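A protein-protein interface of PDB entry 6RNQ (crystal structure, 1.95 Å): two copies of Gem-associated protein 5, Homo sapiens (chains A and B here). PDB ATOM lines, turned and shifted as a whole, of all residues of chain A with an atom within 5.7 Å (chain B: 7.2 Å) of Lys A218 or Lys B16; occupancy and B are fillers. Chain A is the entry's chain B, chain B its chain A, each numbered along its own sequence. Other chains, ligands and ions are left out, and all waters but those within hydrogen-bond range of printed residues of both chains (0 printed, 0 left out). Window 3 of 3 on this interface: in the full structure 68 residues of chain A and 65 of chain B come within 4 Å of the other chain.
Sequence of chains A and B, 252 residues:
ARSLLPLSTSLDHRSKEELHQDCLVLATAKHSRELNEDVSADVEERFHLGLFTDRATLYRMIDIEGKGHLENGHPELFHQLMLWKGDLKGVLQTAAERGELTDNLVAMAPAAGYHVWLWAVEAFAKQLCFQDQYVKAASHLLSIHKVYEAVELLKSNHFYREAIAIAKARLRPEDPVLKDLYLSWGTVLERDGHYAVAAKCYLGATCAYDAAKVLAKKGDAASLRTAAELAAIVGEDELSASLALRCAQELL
Of chain B, only Lys B16 comes within 4 Å of Lys A218.
Of the printed residues of chain A, His B20 touches Leu A215 and Ser A223.
Of the printed residues of chain B, Ala A196 touches Lys B16.
Printed residues of chain B within 4 Å of Leu A215: His B20 (3.7 Å).
Ser B15 touches none of the printed residues of chain A.
The nearest residue of chain B that does not touch Lys A218 is His B20 (6.6 Å).
The nearest printed residue of chain A that does not touch His B20 is Ala A196 (4.2 Å).
CB of Ala A196 touches CE of Lys B16, at 3.6 Å.
CD2 of Leu A215 touches NE2 of His B20, 3.7 Å away.
Lys A218 touches Lys B16 (CE to NZ, 3.6 Å).
Ser A223 touches His B20.
No position is printed for both chains.
Of the 4 pairs that touch across the chains among the printed residues, none has its exchanged pair printed and touching as well.
Hydrophobic or aromatic side chains of chain B within 4 Å of the printed part of chain A: His B20.
Hydrophobic or aromatic side chains of chain A that line the printed part of chain B: Ala A196 and Leu A215.
The side-chain carboxylate of Asp A220 sits at hydrogen-bond distance from the side-chain hydroxyl of Ser A223 (2.4 Å).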
ATOM      1  N   GLY A 193     -23.403 -10.599   1.941  1.00  0.00           N
ATOM      2  CA  GLY A 193     -24.529 -10.041   1.223  1.00  0.00           C
ATOM      3  C   GLY A 193     -24.194  -9.012   0.166  1.00  0.00           C
ATOM      4  O   GLY A 193     -25.115  -8.464  -0.451  1.00  0.00           O
ATOM      5  N   HIS A 194     -22.913  -8.726  -0.064  1.00  0.00           N
ATOM      6  CA  HIS A 194     -22.511  -7.766  -1.094  1.00  0.00           C
ATOM      7  C   HIS A 194     -22.451  -8.508  -2.426  1.00  0.00           C
ATOM      8  O   HIS A 194     -21.388  -8.869  -2.938  1.00  0.00           O
ATOM      9  CB  HIS A 194     -21.184  -7.118  -0.732  1.00  0.00           C
ATOM     10  CG  HIS A 194     -21.184  -6.468   0.616  1.00  0.00           C
ATOM     11  ND1 HIS A 194     -20.802  -7.132   1.762  1.00  0.00           N
ATOM     12  CD2 HIS A 194     -21.533  -5.219   1.003  1.00  0.00           C
ATOM     13  CE1 HIS A 194     -20.908  -6.316   2.796  1.00  0.00           C
ATOM     14  NE2 HIS A 194     -21.349  -5.149   2.363  1.00  0.00           N
ATOM     15  N   TYR A 195     -23.637  -8.731  -2.997  1.00  0.00           N
ATOM     16  CA  TYR A 195     -23.748  -9.594  -4.167  1.00  0.00           C
ATOM     17  C   TYR A 195     -23.206  -8.915  -5.420  1.00  0.00           C
ATOM     18  O   TYR A 195     -22.518  -9.552  -6.225  1.00  0.00           O
ATOM     19  CB  TYR A 195     -25.205 -10.014  -4.356  1.00  0.00           C
ATOM     20  CG  TYR A 195     -25.752 -10.802  -3.183  1.00  0.00           C
ATOM     21  CD1 TYR A 195     -25.352 -12.112  -2.957  1.00  0.00           C
ATOM     22  CD2 TYR A 195     -26.663 -10.235  -2.301  1.00  0.00           C
ATOM     23  CE1 TYR A 195     -25.843 -12.837  -1.887  1.00  0.00           C
ATOM     24  CE2 TYR A 195     -27.162 -10.953  -1.228  1.00  0.00           C
ATOM     25  CZ  TYR A 195     -26.748 -12.254  -1.027  1.00  0.00           C
ATOM     26  OH  TYR A 195     -27.239 -12.975   0.036  1.00  0.00           O
ATOM     27  N   ALA A 196     -23.501  -7.625  -5.606  1.00  0.00           N
ATOM     28  CA  ALA A 196     -22.988  -6.918  -6.776  1.00  0.00           C
ATOM     29  C   ALA A 196     -21.463  -6.912  -6.793  1.00  0.00           C
ATOM     30  O   ALA A 196     -20.845  -7.096  -7.848  1.00  0.00           O
ATOM     31  CB  ALA A 196     -23.530  -5.490  -6.803  1.00  0.00           C
ATOM     32  N   VAL A 214     -24.749 -14.912  -8.630  1.00  0.00           N
ATOM     33  CA  VAL A 214     -24.618 -14.230  -7.345  1.00  0.00           C
ATOM     34  C   VAL A 214     -25.406 -12.925  -7.347  1.00  0.00           C
ATOM     35  O   VAL A 214     -26.028 -12.560  -6.343  1.00  0.00           O
ATOM     36  CB  VAL A 214     -23.131 -14.006  -7.003  1.00  0.00           C
ATOM     37  CG1 VAL A 214     -22.592 -12.749  -7.668  1.00  0.00           C
ATOM     38  CG2 VAL A 214     -22.940 -13.941  -5.496  1.00  0.00           C
ATOM     39  N   LEU A 215     -25.399 -12.201  -8.469  1.00  0.00           N
ATOM     40  CA  LEU A 215     -26.235 -11.010  -8.577  1.00  0.00           C
ATOM     41  C   LEU A 215     -27.705 -11.357  -8.373  1.00  0.00           C
ATOM     42  O   LEU A 215     -28.465 -10.568  -7.799  1.00  0.00           O
ATOM     43  CB  LEU A 215     -26.036 -10.346  -9.939  1.00  0.00           C
ATOM     44  CG  LEU A 215     -25.250  -9.037  -9.978  1.00  0.00           C
ATOM     45  CD1 LEU A 215     -25.123  -8.551 -11.416  1.00  0.00           C
ATOM     46  CD2 LEU A 215     -25.908  -7.977  -9.109  1.00  0.00           C
ATOM     47  N   ALA A 216     -28.123 -12.536  -8.838  1.00  0.00           N
ATOM     48  CA  ALA A 216     -29.522 -12.927  -8.714  1.00  0.00           C
ATOM     49  C   ALA A 216     -29.894 -13.257  -7.275  1.00  0.00           C
ATOM     50  O   ALA A 216     -31.069 -13.150  -6.903  1.00  0.00           O
ATOM     51  CB  ALA A 216     -29.812 -14.125  -9.619  1.00  0.00           C
ATOM     52  N   LYS A 217     -28.920 -13.652  -6.451  1.00  0.00           N
ATOM     53  CA  LYS A 217     -29.229 -14.021  -5.074  1.00  0.00           C
ATOM     54  C   LYS A 217     -29.857 -12.873  -4.297  1.00  0.00           C
ATOM     55  O   LYS A 217     -30.558 -13.121  -3.309  1.00  0.00           O
ATOM     56  CB  LYS A 217     -27.969 -14.501  -4.354  1.00  0.00           C
ATOM     57  CG  LYS A 217     -27.470 -15.861  -4.811  1.00  0.00           C
ATOM     58  CD  LYS A 217     -26.683 -16.547  -3.704  1.00  0.00           C
ATOM     59  CE  LYS A 217     -26.093 -17.867  -4.167  1.00  0.00           C
ATOM     60  NZ  LYS A 217     -25.383 -18.567  -3.060  1.00  0.00           N
ATOM     61  N   LYS A 218     -29.625 -11.626  -4.713  1.00  0.00           N
ATOM     62  CA  LYS A 218     -30.257 -10.498  -4.037  1.00  0.00           C
ATOM     63  C   LYS A 218     -31.773 -10.642  -4.045  1.00  0.00           C
ATOM     64  O   LYS A 218     -32.432 -10.407  -3.025  1.00  0.00           O
ATOM     65  CB  LYS A 218     -29.832  -9.187  -4.699  1.00  0.00           C
ATOM     66  CG  LYS A 218     -30.206  -7.930  -3.915  1.00  0.00           C
ATOM     67  CD  LYS A 218     -29.648  -7.963  -2.498  1.00  0.00           C
ATOM     68  CE  LYS A 218     -29.413  -6.565  -1.943  1.00  0.00           C
ATOM     69  NZ  LYS A 218     -30.673  -5.814  -1.692  1.00  0.00           N
ATOM     70  N   GLY A 219     -32.344 -11.032  -5.184  1.00  0.00           N
ATOM     71  CA  GLY A 219     -33.752 -11.344  -5.285  1.00  0.00           C
ATOM     72  C   GLY A 219     -34.625 -10.229  -5.820  1.00  0.00           C
ATOM     73  O   GLY A 219     -35.783 -10.491  -6.172  1.00  0.00           O
ATOM     74  N   ASP A 220     -34.116  -9.004  -5.893  1.00  0.00           N
ATOM     75  CA  ASP A 220     -34.915  -7.887  -6.369  1.00  0.00           C
ATOM     76  C   ASP A 220     -34.923  -7.844  -7.894  1.00  0.00           C
ATOM     77  O   ASP A 220     -34.106  -8.478  -8.568  1.00  0.00           O
ATOM     78  CB  ASP A 220     -34.382  -6.569  -5.807  1.00  0.00           C
ATOM     79  CG  ASP A 220     -33.025  -6.205  -6.368  1.00  0.00           C
ATOM     80  OD1 ASP A 220     -32.975  -5.465  -7.371  1.00  0.00           O
ATOM     81  OD2 ASP A 220     -32.007  -6.668  -5.814  1.00  0.00           O
ATOM     82  N   SER A 223     -31.668  -6.427  -9.669  1.00  0.00           N
ATOM     83  CA  SER A 223     -30.543  -7.356  -9.693  1.00  0.00           C
ATOM     84  C   SER A 223     -30.791  -8.505 -10.664  1.00  0.00           C
ATOM     85  O   SER A 223     -29.856  -8.988 -11.311  1.00  0.00           O
ATOM     86  CB  SER A 223     -30.279  -7.898  -8.288  1.00  0.00           C
ATOM     87  OG  SER A 223     -30.114  -6.842  -7.359  1.00  0.00           O
ATOM     88  N   HIS B  13     -17.908   2.072  -3.843  1.00  0.00           N
ATOM     89  CA  HIS B  13     -18.908   2.180  -2.784  1.00  0.00           C
ATOM     90  C   HIS B  13     -19.999   3.182  -3.149  1.00  0.00           C
ATOM     91  O   HIS B  13     -20.509   3.913  -2.302  1.00  0.00           O
ATOM     92  CB  HIS B  13     -18.257   2.563  -1.456  1.00  0.00           C
ATOM     93  CG  HIS B  13     -17.535   1.432  -0.793  1.00  0.00           C
ATOM     94  ND1 HIS B  13     -16.346   0.925  -1.272  1.00  0.00           N
ATOM     95  CD2 HIS B  13     -17.834   0.706   0.311  1.00  0.00           C
ATOM     96  CE1 HIS B  13     -15.942  -0.061  -0.491  1.00  0.00           C
ATOM     97  NE2 HIS B  13     -16.827  -0.214   0.477  1.00  0.00           N
ATOM     98  N   ARG B  14     -20.361   3.230  -4.420  1.00  0.00           N
ATOM     99  CA  ARG B  14     -21.447   4.080  -4.877  1.00  0.00           C
ATOM    100  C   ARG B  14     -22.760   3.291  -4.845  1.00  0.00           C
ATOM    101  O   ARG B  14     -22.818   2.163  -4.345  1.00  0.00           O
ATOM    102  CB  ARG B  14     -21.128   4.622  -6.268  1.00  0.00           C
ATOM    103  CG  ARG B  14     -19.917   5.540  -6.310  1.00  0.00           C
ATOM    104  CD  ARG B  14     -19.708   6.143  -7.699  1.00  0.00           C
ATOM    105  NE  ARG B  14     -19.260   5.153  -8.679  1.00  0.00           N
ATOM    106  CZ  ARG B  14     -19.044   5.411  -9.966  1.00  0.00           C
ATOM    107  NH1 ARG B  14     -18.637   4.449 -10.784  1.00  0.00           N
ATOM    108  NH2 ARG B  14     -19.236   6.635 -10.440  1.00  0.00           N
ATOM    109  N   SER B  15     -23.830   3.879  -5.380  1.00  0.00           N
ATOM    110  CA  SER B  15     -25.119   3.200  -5.417  1.00  0.00           C
ATOM    111  C   SER B  15     -25.021   1.908  -6.222  1.00  0.00           C
ATOM    112  O   SER B  15     -24.220   1.784  -7.153  1.00  0.00           O
ATOM    113  CB  SER B  15     -26.184   4.109  -6.027  1.00  0.00           C
ATOM    114  OG  SER B  15     -26.001   4.235  -7.438  1.00  0.00           O
ATOM    115  N   LYS B  16     -25.853   0.928  -5.856  1.00  0.00           N
ATOM    116  CA  LYS B  16     -25.803  -0.356  -6.544  1.00  0.00           C
ATOM    117  C   LYS B  16     -26.271  -0.249  -7.987  1.00  0.00           C
ATOM    118  O   LYS B  16     -25.932  -1.120  -8.790  1.00  0.00           O
ATOM    119  CB  LYS B  16     -26.614  -1.399  -5.780  1.00  0.00           C
ATOM    120  CG  LYS B  16     -25.917  -1.841  -4.485  1.00  0.00           C
ATOM    121  CD  LYS B  16     -26.550  -3.081  -3.859  1.00  0.00           C
ATOM    122  CE  LYS B  16     -26.225  -4.349  -4.657  1.00  0.00           C
ATOM    123  NZ  LYS B  16     -26.491  -5.612  -3.876  1.00  0.00           N
ATOM    124  N   GLU B  17     -27.022   0.798  -8.340  1.00  0.00           N
ATOM    125  CA  GLU B  17     -27.263   1.078  -9.751  1.00  0.00           C
ATOM    126  C   GLU B  17     -25.944   1.313 -10.475  1.00  0.00           C
ATOM    127  O   GLU B  17     -25.749   0.865 -11.609  1.00  0.00           O
ATOM    128  CB  GLU B  17     -28.179   2.295  -9.907  1.00  0.00           C
ATOM    129  CG  GLU B  17     -29.554   2.145  -9.258  1.00  0.00           C
ATOM    130  CD  GLU B  17     -29.588   2.673  -7.829  1.00  0.00           C
ATOM    131  OE1 GLU B  17     -28.901   3.686  -7.530  1.00  0.00           O
ATOM    132  OE2 GLU B  17     -30.305   2.065  -6.999  1.00  0.00           O
ATOM    133  N   GLU B  18     -25.025   2.026  -9.831  1.00  0.00           N
ATOM    134  CA  GLU B  18     -23.702   2.236 -10.402  1.00  0.00           C
ATOM    135  C   GLU B  18     -22.915   0.934 -10.451  1.00  0.00           C
ATOM    136  O   GLU B  18     -22.229   0.655 -11.441  1.00  0.00           O
ATOM    137  CB  GLU B  18     -22.960   3.294  -9.580  1.00  0.00           C
ATOM    138  CG  GLU B  18     -21.993   4.133 -10.384  1.00  0.00           C
ATOM    139  CD  GLU B  18     -22.687   5.064 -11.352  1.00  0.00           C
ATOM    140  OE1 GLU B  18     -23.729   5.634 -10.976  1.00  0.00           O
ATOM    141  OE2 GLU B  18     -22.187   5.217 -12.483  1.00  0.00           O
ATOM    142  N   LEU B  19     -23.005   0.115  -9.401  1.00  0.00           N
ATOM    143  CA  LEU B  19     -22.295  -1.158  -9.397  1.00  0.00           C
ATOM    144  C   LEU B  19     -22.874  -2.123 -10.429  1.00  0.00           C
ATOM    145  O   LEU B  19     -22.160  -3.002 -10.929  1.00  0.00           O
ATOM    146  CB  LEU B  19     -22.352  -1.796  -8.010  1.00  0.00           C
ATOM    147  CG  LEU B  19     -21.650  -1.063  -6.859  1.00  0.00           C
ATOM    148  CD1 LEU B  19     -21.771  -1.884  -5.555  1.00  0.00           C
ATOM    149  CD2 LEU B  19     -20.189  -0.785  -7.178  1.00  0.00           C
ATOM    150  N   HIS B  20     -24.167  -2.000 -10.743  1.00  0.00           N
ATOM    151  CA  HIS B  20     -24.741  -2.834 -11.794  1.00  0.00           C
ATOM    152  C   HIS B  20     -24.174  -2.458 -13.156  1.00  0.00           C
ATOM    153  O   HIS B  20     -23.876  -3.341 -13.966  1.00  0.00           O
ATOM    154  CB  HIS B  20     -26.266  -2.734 -11.776  1.00  0.00           C
ATOM    155  CG  HIS B  20     -26.890  -3.449 -10.620  1.00  0.00           C
ATOM    156  ND1 HIS B  20     -28.251  -3.564 -10.460  1.00  0.00           N
ATOM    157  CD2 HIS B  20     -26.334  -4.074  -9.552  1.00  0.00           C
ATOM    158  CE1 HIS B  20     -28.510  -4.240  -9.354  1.00  0.00           C
ATOM    159  NE2 HIS B  20     -27.363  -4.562  -8.783  1.00  0.00           N
ATOM    160  N   GLN B  21     -24.004  -1.159 -13.422  1.00  0.00           N
ATOM    161  CA  GLN B  21     -23.317  -0.747 -14.643  1.00  0.00           C
ATOM    162  C   GLN B  21     -21.876  -1.248 -14.656  1.00  0.00           C
ATOM    163  O   GLN B  21     -21.382  -1.700 -15.698  1.00  0.00           O
ATOM    164  CB  GLN B  21     -23.351   0.771 -14.785  1.00  0.00           C
ATOM    165  CG  GLN B  21     -24.661   1.311 -15.285  1.00  0.00           C
ATOM    166  CD  GLN B  21     -25.010   0.787 -16.679  1.00  0.00           C
ATOM    167  OE1 GLN B  21     -24.177   0.805 -17.598  1.00  0.00           O
ATOM    168  NE2 GLN B  21     -26.230   0.306 -16.837  1.00  0.00           N
ATOM    169  N   ASP B  22     -21.187  -1.171 -13.506  1.00  0.00           N
ATOM    170  CA  ASP B  22     -19.853  -1.755 -13.393  1.00  0.00           C
ATOM    171  C   ASP B  22     -19.855  -3.197 -13.891  1.00  0.00           C
ATOM    172  O   ASP B  22     -19.003  -3.593 -14.690  1.00  0.00           O
ATOM    173  CB  ASP B  22     -19.367  -1.713 -11.938  1.00  0.00           C
ATOM    174  CG  ASP B  22     -18.878  -0.324 -11.496  1.00  0.00           C
ATOM    175  OD1 ASP B  22     -18.818   0.617 -12.321  1.00  0.00           O
ATOM    176  OD2 ASP B  22     -18.539  -0.170 -10.298  1.00  0.00           O
